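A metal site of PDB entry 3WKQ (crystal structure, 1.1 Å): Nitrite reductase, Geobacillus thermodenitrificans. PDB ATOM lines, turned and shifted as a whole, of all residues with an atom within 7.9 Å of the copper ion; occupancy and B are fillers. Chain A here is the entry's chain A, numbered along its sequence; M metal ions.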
ATOM      1  N   ALA A  47      27.820 -12.020 -11.934  1.00  0.00           N
ATOM      2  CA  ALA A  47      26.637 -12.603 -11.268  1.00  0.00           C
ATOM      3  C   ALA A  47      27.023 -12.707  -9.798  1.00  0.00           C
ATOM      4  O   ALA A  47      28.099 -13.233  -9.459  1.00  0.00           O
ATOM      5  CB  ALA A  47      26.338 -13.980 -11.835  1.00  0.00           C
ATOM      6  N   TRP A  63      19.586 -12.794  -6.371  1.00  0.00           N
ATOM      7  CA  TRP A  63      20.532 -13.238  -7.409  1.00  0.00           C
ATOM      8  C   TRP A  63      20.575 -12.091  -8.379  1.00  0.00           C
ATOM      9  O   TRP A  63      19.543 -11.670  -8.895  1.00  0.00           O
ATOM     10  CB  TRP A  63      20.034 -14.518  -8.070  1.00  0.00           C
ATOM     11  CG  TRP A  63      19.859 -15.698  -7.168  1.00  0.00           C
ATOM     12  CD1 TRP A  63      19.907 -15.788  -5.797  1.00  0.00           C
ATOM     13  CD2 TRP A  63      19.598 -17.016  -7.632  1.00  0.00           C
ATOM     14  NE1 TRP A  63      19.712 -17.091  -5.382  1.00  0.00           N
ATOM     15  CE2 TRP A  63      19.496 -17.868  -6.489  1.00  0.00           C
ATOM     16  CE3 TRP A  63      19.325 -17.567  -8.906  1.00  0.00           C
ATOM     17  CZ2 TRP A  63      19.212 -19.228  -6.601  1.00  0.00           C
ATOM     18  CZ3 TRP A  63      19.040 -18.911  -8.961  1.00  0.00           C
ATOM     19  CH2 TRP A  63      18.955 -19.753  -7.844  1.00  0.00           C
ATOM     20  N   THR A  64      21.791 -11.574  -8.674  1.00  0.00           N
ATOM     21  CA  THR A  64      21.891 -10.307  -9.392  1.00  0.00           C
ATOM     22  C   THR A  64      22.974 -10.330 -10.417  1.00  0.00           C
ATOM     23  O   THR A  64      23.970 -11.085 -10.306  1.00  0.00           O
ATOM     24  CB  THR A  64      22.157  -9.134  -8.410  1.00  0.00           C
ATOM     25  OG1 THR A  64      23.545  -9.157  -7.999  1.00  0.00           O
ATOM     26  CG2 THR A  64      21.263  -9.092  -7.220  1.00  0.00           C
ATOM     27  N   PHE A  65      22.879  -9.366 -11.323  1.00  0.00           N
ATOM     28  CA  PHE A  65      24.015  -8.872 -12.065  1.00  0.00           C
ATOM     29  C   PHE A  65      24.541  -7.657 -11.308  1.00  0.00           C
ATOM     30  O   PHE A  65      23.842  -6.664 -11.099  1.00  0.00           O
ATOM     31  CB  PHE A  65      23.614  -8.482 -13.489  1.00  0.00           C
ATOM     32  CG  PHE A  65      23.168  -9.679 -14.304  1.00  0.00           C
ATOM     33  CD1 PHE A  65      24.098 -10.642 -14.739  1.00  0.00           C
ATOM     34  CD2 PHE A  65      21.802  -9.867 -14.556  1.00  0.00           C
ATOM     35  CE1 PHE A  65      23.660 -11.708 -15.518  1.00  0.00           C
ATOM     36  CE2 PHE A  65      21.391 -10.953 -15.367  1.00  0.00           C
ATOM     37  CZ  PHE A  65      22.317 -11.889 -15.810  1.00  0.00           C
ATOM     38  N   LEU A  86      30.834 -12.437 -18.537  1.00  0.00           N
ATOM     39  CA  LEU A  86      30.179 -12.635 -17.227  1.00  0.00           C
ATOM     40  C   LEU A  86      31.182 -13.269 -16.300  1.00  0.00           C
ATOM     41  O   LEU A  86      31.700 -14.364 -16.605  1.00  0.00           O
ATOM     42  CB  LEU A  86      28.950 -13.539 -17.401  1.00  0.00           C
ATOM     43  CG  LEU A  86      28.148 -13.721 -16.084  1.00  0.00           C
ATOM     44  CD1 LEU A  86      27.577 -12.414 -15.560  1.00  0.00           C
ATOM     45  CD2 LEU A  86      27.042 -14.770 -16.315  1.00  0.00           C
ATOM     46  N   ASN A  88      31.190 -15.056 -12.812  1.00  0.00           N
ATOM     47  CA  ASN A  88      30.213 -15.623 -11.873  1.00  0.00           C
ATOM     48  C   ASN A  88      30.862 -15.683 -10.472  1.00  0.00           C
ATOM     49  O   ASN A  88      31.768 -16.511 -10.232  1.00  0.00           O
ATOM     50  CB  ASN A  88      29.775 -17.021 -12.335  1.00  0.00           C
ATOM     51  CG  ASN A  88      28.657 -17.541 -11.463  1.00  0.00           C
ATOM     52  OD1 ASN A  88      28.241 -16.864 -10.531  1.00  0.00           O
ATOM     53  ND2 ASN A  88      28.202 -18.744 -11.734  1.00  0.00           N
ATOM     54  N   ASP A  90      28.883 -16.213  -7.793  1.00  0.00           N
ATOM     55  CA  ASP A  90      28.054 -17.085  -6.959  1.00  0.00           C
ATOM     56  C   ASP A  90      28.913 -18.309  -6.569  1.00  0.00           C
ATOM     57  O   ASP A  90      29.492 -18.943  -7.469  1.00  0.00           O
ATOM     58  CB  ASP A  90      26.837 -17.507  -7.760  1.00  0.00           C
ATOM     59  CG  ASP A  90      25.779 -18.235  -6.972  1.00  0.00           C
ATOM     60  OD1 ASP A  90      26.153 -19.137  -6.134  1.00  0.00           O
ATOM     61  OD2 ASP A  90      24.588 -17.988  -7.208  1.00  0.00           O
ATOM     62  N   VAL A  93      25.934 -21.626  -7.689  1.00  0.00           N
ATOM     63  CA  VAL A  93      24.959 -21.735  -8.801  1.00  0.00           C
ATOM     64  C   VAL A  93      25.589 -21.202 -10.073  1.00  0.00           C
ATOM     65  O   VAL A  93      26.121 -20.091 -10.084  1.00  0.00           O
ATOM     66  CB  VAL A  93      23.637 -20.989  -8.487  1.00  0.00           C
ATOM     67  CG1 VAL A  93      22.584 -21.256  -9.508  1.00  0.00           C
ATOM     68  CG2 VAL A  93      23.119 -21.338  -7.080  1.00  0.00           C
ATOM     69  N   PRO A  94      25.435 -21.919 -11.215  1.00  0.00           N
ATOM     70  CA  PRO A  94      25.860 -21.328 -12.535  1.00  0.00           C
ATOM     71  C   PRO A  94      24.878 -20.202 -12.937  1.00  0.00           C
ATOM     72  O   PRO A  94      23.704 -20.239 -12.525  1.00  0.00           O
ATOM     73  CB  PRO A  94      25.670 -22.509 -13.508  1.00  0.00           C
ATOM     74  CG  PRO A  94      25.761 -23.748 -12.573  1.00  0.00           C
ATOM     75  CD  PRO A  94      25.008 -23.323 -11.321  1.00  0.00           C
ATOM     76  N   HIS A  95      25.393 -19.303 -13.762  1.00  0.00           N
ATOM     77  CA  HIS A  95      24.569 -18.222 -14.307  1.00  0.00           C
ATOM     78  C   HIS A  95      24.967 -17.947 -15.722  1.00  0.00           C
ATOM     79  O   HIS A  95      26.029 -18.401 -16.198  1.00  0.00           O
ATOM     80  CB  HIS A  95      24.746 -16.933 -13.412  1.00  0.00           C
ATOM     81  CG  HIS A  95      24.257 -17.101 -12.066  1.00  0.00           C
ATOM     82  ND1 HIS A  95      22.930 -17.233 -11.740  1.00  0.00           N
ATOM     83  CD2 HIS A  95      24.913 -17.219 -10.867  1.00  0.00           C
ATOM     84  CE1 HIS A  95      22.804 -17.409 -10.466  1.00  0.00           C
ATOM     85  NE2 HIS A  95      23.989 -17.421  -9.881  1.00  0.00           N
ATOM     86  N   SER A  96      24.168 -17.171 -16.429  1.00  0.00           N
ATOM     87  CA  SER A  96      24.366 -16.927 -17.838  1.00  0.00           C
ATOM     88  C   SER A  96      23.743 -15.566 -18.196  1.00  0.00           C
ATOM     89  O   SER A  96      23.187 -14.893 -17.327  1.00  0.00           O
ATOM     90  CB  SER A  96      23.735 -18.029 -18.662  1.00  0.00           C
ATOM     91  OG  SER A  96      22.334 -18.142 -18.386  1.00  0.00           O
ATOM     92  N   MET A  97      23.797 -15.205 -19.464  1.00  0.00           N
ATOM     93  CA  MET A  97      23.210 -13.921 -19.899  1.00  0.00           C
ATOM     94  C   MET A  97      22.577 -14.113 -21.252  1.00  0.00           C
ATOM     95  O   MET A  97      23.172 -14.625 -22.228  1.00  0.00           O
ATOM     96  CB  MET A  97      24.322 -12.855 -20.050  1.00  0.00           C
ATOM     97  CG  MET A  97      23.859 -11.598 -20.671  1.00  0.00           C
ATOM     98  SD  MET A  97      22.560 -10.723 -19.724  1.00  0.00           S
ATOM     99  CE  MET A  97      23.612  -9.825 -18.607  1.00  0.00           C
ATOM    100  N   ASP A 112      25.916 -21.403 -19.688  1.00  0.00           N
ATOM    101  CA  ASP A 112      26.268 -21.185 -18.298  1.00  0.00           C
ATOM    102  C   ASP A 112      27.739 -20.908 -18.102  1.00  0.00           C
ATOM    103  O   ASP A 112      28.610 -21.464 -18.771  1.00  0.00           O
ATOM    104  CB  ASP A 112      25.858 -22.435 -17.482  1.00  0.00           C
ATOM    105  CG  ASP A 112      24.359 -22.589 -17.368  1.00  0.00           C
ATOM    106  OD1 ASP A 112      23.610 -21.649 -17.641  1.00  0.00           O
ATOM    107  OD2 ASP A 112      23.957 -23.715 -17.021  1.00  0.00           O
ATOM    108  N   VAL A 113      28.010 -20.091 -17.091  1.00  0.00           N
ATOM    109  CA  VAL A 113      29.335 -19.806 -16.534  1.00  0.00           C
ATOM    110  C   VAL A 113      29.320 -20.380 -15.155  1.00  0.00           C
ATOM    111  O   VAL A 113      28.446 -20.056 -14.333  1.00  0.00           O
ATOM    112  CB  VAL A 113      29.609 -18.315 -16.557  1.00  0.00           C
ATOM    113  CG1 VAL A 113      30.965 -18.024 -15.872  1.00  0.00           C
ATOM    114  CG2 VAL A 113      29.582 -17.765 -17.923  1.00  0.00           C
ATOM    115  N   HIS A 134      18.449 -10.938 -19.206  1.00  0.00           N
ATOM    116  CA  HIS A 134      18.248 -11.729 -18.007  1.00  0.00           C
ATOM    117  C   HIS A 134      19.136 -12.950 -18.027  1.00  0.00           C
ATOM    118  O   HIS A 134      19.652 -13.360 -19.073  1.00  0.00           O
ATOM    119  CB  HIS A 134      16.772 -12.173 -17.902  1.00  0.00           C
ATOM    120  CG  HIS A 134      16.267 -12.956 -19.053  1.00  0.00           C
ATOM    121  ND1 HIS A 134      16.421 -14.334 -19.158  1.00  0.00           N
ATOM    122  CD2 HIS A 134      15.590 -12.596 -20.153  1.00  0.00           C
ATOM    123  CE1 HIS A 134      15.827 -14.729 -20.309  1.00  0.00           C
ATOM    124  NE2 HIS A 134      15.294 -13.694 -20.938  1.00  0.00           N
ATOM    125  N   CYS A 135      19.311 -13.557 -16.860  1.00  0.00           N
ATOM    126  CA  CYS A 135      19.980 -14.865 -16.807  1.00  0.00           C
ATOM    127  C   CYS A 135      19.169 -15.897 -17.571  1.00  0.00           C
ATOM    128  O   CYS A 135      17.929 -15.908 -17.464  1.00  0.00           O
ATOM    129  CB  CYS A 135      20.206 -15.252 -15.352  1.00  0.00           C
ATOM    130  SG  CYS A 135      21.033 -16.828 -15.174  1.00  0.00           S
ATOM    131  N   GLY A 136      19.841 -16.765 -18.279  1.00  0.00           N
ATOM    132  CA  GLY A 136      19.214 -17.822 -19.050  1.00  0.00           C
ATOM    133  C   GLY A 136      19.457 -19.233 -18.528  1.00  0.00           C
ATOM    134  O   GLY A 136      19.326 -20.189 -19.303  1.00  0.00           O
ATOM    135  N   THR A 137      19.810 -19.364 -17.260  1.00  0.00           N
ATOM    136  CA  THR A 137      20.123 -20.683 -16.692  1.00  0.00           C
ATOM    137  C   THR A 137      18.845 -21.361 -16.222  1.00  0.00           C
ATOM    138  O   THR A 137      17.976 -20.775 -15.582  1.00  0.00           O
ATOM    139  CB  THR A 137      21.113 -20.497 -15.554  1.00  0.00           C
ATOM    140  OG1 THR A 137      22.309 -19.881 -16.090  1.00  0.00           O
ATOM    141  CG2 THR A 137      21.468 -21.776 -14.823  1.00  0.00           C
ATOM    142  N   LYS A 138      18.717 -22.675 -16.540  1.00  0.00           N
ATOM    143  CA  LYS A 138      17.546 -23.442 -16.154  1.00  0.00           C
ATOM    144  C   LYS A 138      17.552 -23.626 -14.623  1.00  0.00           C
ATOM    145  O   LYS A 138      18.587 -23.988 -14.033  1.00  0.00           O
ATOM    146  CB  LYS A 138      17.671 -24.804 -16.827  1.00  0.00           C
ATOM    147  CG  LYS A 138      16.486 -25.690 -16.505  1.00  0.00           C
ATOM    148  CD  LYS A 138      16.602 -26.940 -17.301  1.00  0.00           C
ATOM    149  CE  LYS A 138      16.295 -26.676 -18.776  1.00  0.00           C
ATOM    150  NZ  LYS A 138      15.652 -27.871 -19.397  1.00  0.00           N
ATOM    151  N   PRO A 139      16.423 -23.523 -13.937  1.00  0.00           N
ATOM    152  CA  PRO A 139      15.126 -23.029 -14.467  1.00  0.00           C
ATOM    153  C   PRO A 139      15.132 -21.514 -14.617  1.00  0.00           C
ATOM    154  O   PRO A 139      15.402 -20.799 -13.622  1.00  0.00           O
ATOM    155  CB  PRO A 139      14.082 -23.418 -13.369  1.00  0.00           C
ATOM    156  CG  PRO A 139      14.868 -24.172 -12.353  1.00  0.00           C
ATOM    157  CD  PRO A 139      16.280 -23.888 -12.533  1.00  0.00           C
ATOM    158  N   VAL A 140      14.831 -21.028 -15.798  1.00  0.00           N
ATOM    159  CA  VAL A 140      14.958 -19.590 -16.023  1.00  0.00           C
ATOM    160  C   VAL A 140      14.031 -18.809 -15.139  1.00  0.00           C
ATOM    161  O   VAL A 140      14.388 -17.739 -14.635  1.00  0.00           O
ATOM    162  CB  VAL A 140      14.719 -19.289 -17.534  1.00  0.00           C
ATOM    163  CG1 VAL A 140      14.686 -17.795 -17.811  1.00  0.00           C
ATOM    164  CG2 VAL A 140      15.873 -19.965 -18.335  1.00  0.00           C
ATOM    165  N   GLN A 142      13.352 -19.329 -12.068  1.00  0.00           N
ATOM    166  CA  GLN A 142      14.003 -19.149 -10.791  1.00  0.00           C
ATOM    167  C   GLN A 142      15.039 -18.019 -10.832  1.00  0.00           C
ATOM    168  O   GLN A 142      15.131 -17.192  -9.942  1.00  0.00           O
ATOM    169  CB  GLN A 142      14.628 -20.464 -10.380  1.00  0.00           C
ATOM    170  CG  GLN A 142      15.250 -20.400  -9.026  1.00  0.00           C
ATOM    171  CD  GLN A 142      15.801 -21.737  -8.570  1.00  0.00           C
ATOM    172  OE1 GLN A 142      16.058 -22.639  -9.374  1.00  0.00           O
ATOM    173  NE2 GLN A 142      15.988 -21.867  -7.259  1.00  0.00           N
ATOM    174  N   HIS A 143      15.859 -18.028 -11.896  1.00  0.00           N
ATOM    175  CA  HIS A 143      16.914 -17.030 -12.015  1.00  0.00           C
ATOM    176  C   HIS A 143      16.299 -15.620 -12.210  1.00  0.00           C
ATOM    177  O   HIS A 143      16.791 -14.647 -11.552  1.00  0.00           O
ATOM    178  CB  HIS A 143      17.875 -17.418 -13.076  1.00  0.00           C
ATOM    179  CG  HIS A 143      18.697 -18.607 -12.670  1.00  0.00           C
ATOM    180  ND1 HIS A 143      20.070 -18.456 -12.344  1.00  0.00           N
ATOM    181  CD2 HIS A 143      18.397 -19.935 -12.563  1.00  0.00           C
ATOM    182  CE1 HIS A 143      20.489 -19.679 -12.067  1.00  0.00           C
ATOM    183  NE2 HIS A 143      19.530 -20.596 -12.131  1.00  0.00           N
ATOM    184  N   ILE A 144      15.300 -15.491 -13.082  1.00  0.00           N
ATOM    185  CA  ILE A 144      14.695 -14.204 -13.245  1.00  0.00           C
ATOM    186  C   ILE A 144      14.011 -13.775 -11.943  1.00  0.00           C
ATOM    187  O   ILE A 144      14.218 -12.634 -11.468  1.00  0.00           O
ATOM    188  CB  ILE A 144      13.686 -14.181 -14.423  1.00  0.00           C
ATOM    189  CG1 ILE A 144      14.361 -14.473 -15.737  1.00  0.00           C
ATOM    190  CG2 ILE A 144      13.019 -12.821 -14.456  1.00  0.00           C
ATOM    191  CD1 ILE A 144      13.424 -14.547 -16.927  1.00  0.00           C
ATOM    192  N   ASN A 146      14.506 -14.435  -8.893  1.00  0.00           N
ATOM    193  CA  ASN A 146      15.404 -14.091  -7.827  1.00  0.00           C
ATOM    194  C   ASN A 146      16.184 -12.755  -8.071  1.00  0.00           C
ATOM    195  O   ASN A 146      16.868 -12.349  -7.160  1.00  0.00           O
ATOM    196  CB  ASN A 146      16.374 -15.223  -7.515  1.00  0.00           C
ATOM    197  CG  ASN A 146      15.775 -16.325  -6.700  1.00  0.00           C
ATOM    198  OD1 ASN A 146      14.913 -16.091  -5.813  1.00  0.00           O
ATOM    199  ND2 ASN A 146      16.228 -17.551  -6.908  1.00  0.00           N
ATOM    200  N   GLY A 147      16.046 -12.166  -9.266  1.00  0.00           N
ATOM    201  CA  GLY A 147      16.548 -10.840  -9.517  1.00  0.00           C
ATOM    202  C   GLY A 147      17.401 -10.670 -10.750  1.00  0.00           C
ATOM    203  O   GLY A 147      17.839  -9.542 -10.981  1.00  0.00           O
ATOM    204  N   MET A 148      17.628 -11.718 -11.578  1.00  0.00           N
ATOM    205  CA  MET A 148      18.587 -11.607 -12.661  1.00  0.00           C
ATOM    206  C   MET A 148      17.899 -11.125 -13.949  1.00  0.00           C
ATOM    207  O   MET A 148      17.689 -11.890 -14.893  1.00  0.00           O
ATOM    208  CB  MET A 148      19.245 -12.968 -12.857  1.00  0.00           C
ATOM    209  CG  MET A 148      19.901 -13.430 -11.586  1.00  0.00           C
ATOM    210  SD  MET A 148      21.140 -14.743 -11.733  1.00  0.00           S
ATOM    211  CE  MET A 148      22.508 -13.800 -12.415  1.00  0.00           C
HETATM  212 CU    CU M   1      21.315 -17.019 -12.978  1.00  0.00          CU
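NE2 of His 95 lies close to O of Val 93, 3.4 Å away. A ring nitrogen (NE2) of His 95 is in hydrogen-bond range of the side-chain carboxylate (OD2) of Asp 90 (2.8 Å). O of His 95 sits at hydrogen-bond distance from N of Val 113 (2.8 Å). The side-chain hydroxyl (OG1) of Thr 137 lies close to the side-chain sulfur (SG) of Cys 135 (3.4 Å). The side-chain sulfur of Cys 135 sits close to the backbone NH of Ser 96. The backbone carbonyl oxygen of Trp 63 lies close to the backbone NH of Met 148 (3.3 Å).
Four residues have an atom within 4 Å of the copper ion: His 95, Cys 135, His 143 and Met 148.
The copper ion is bound by ND1 of His 143 (2.0 Å), ND1 of His 95 (2.0 Å), SG of Cys 135 (2.2 Å) and SD of Met 148 (2.6 Å). The copper ion has four donor atoms within binding distance.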
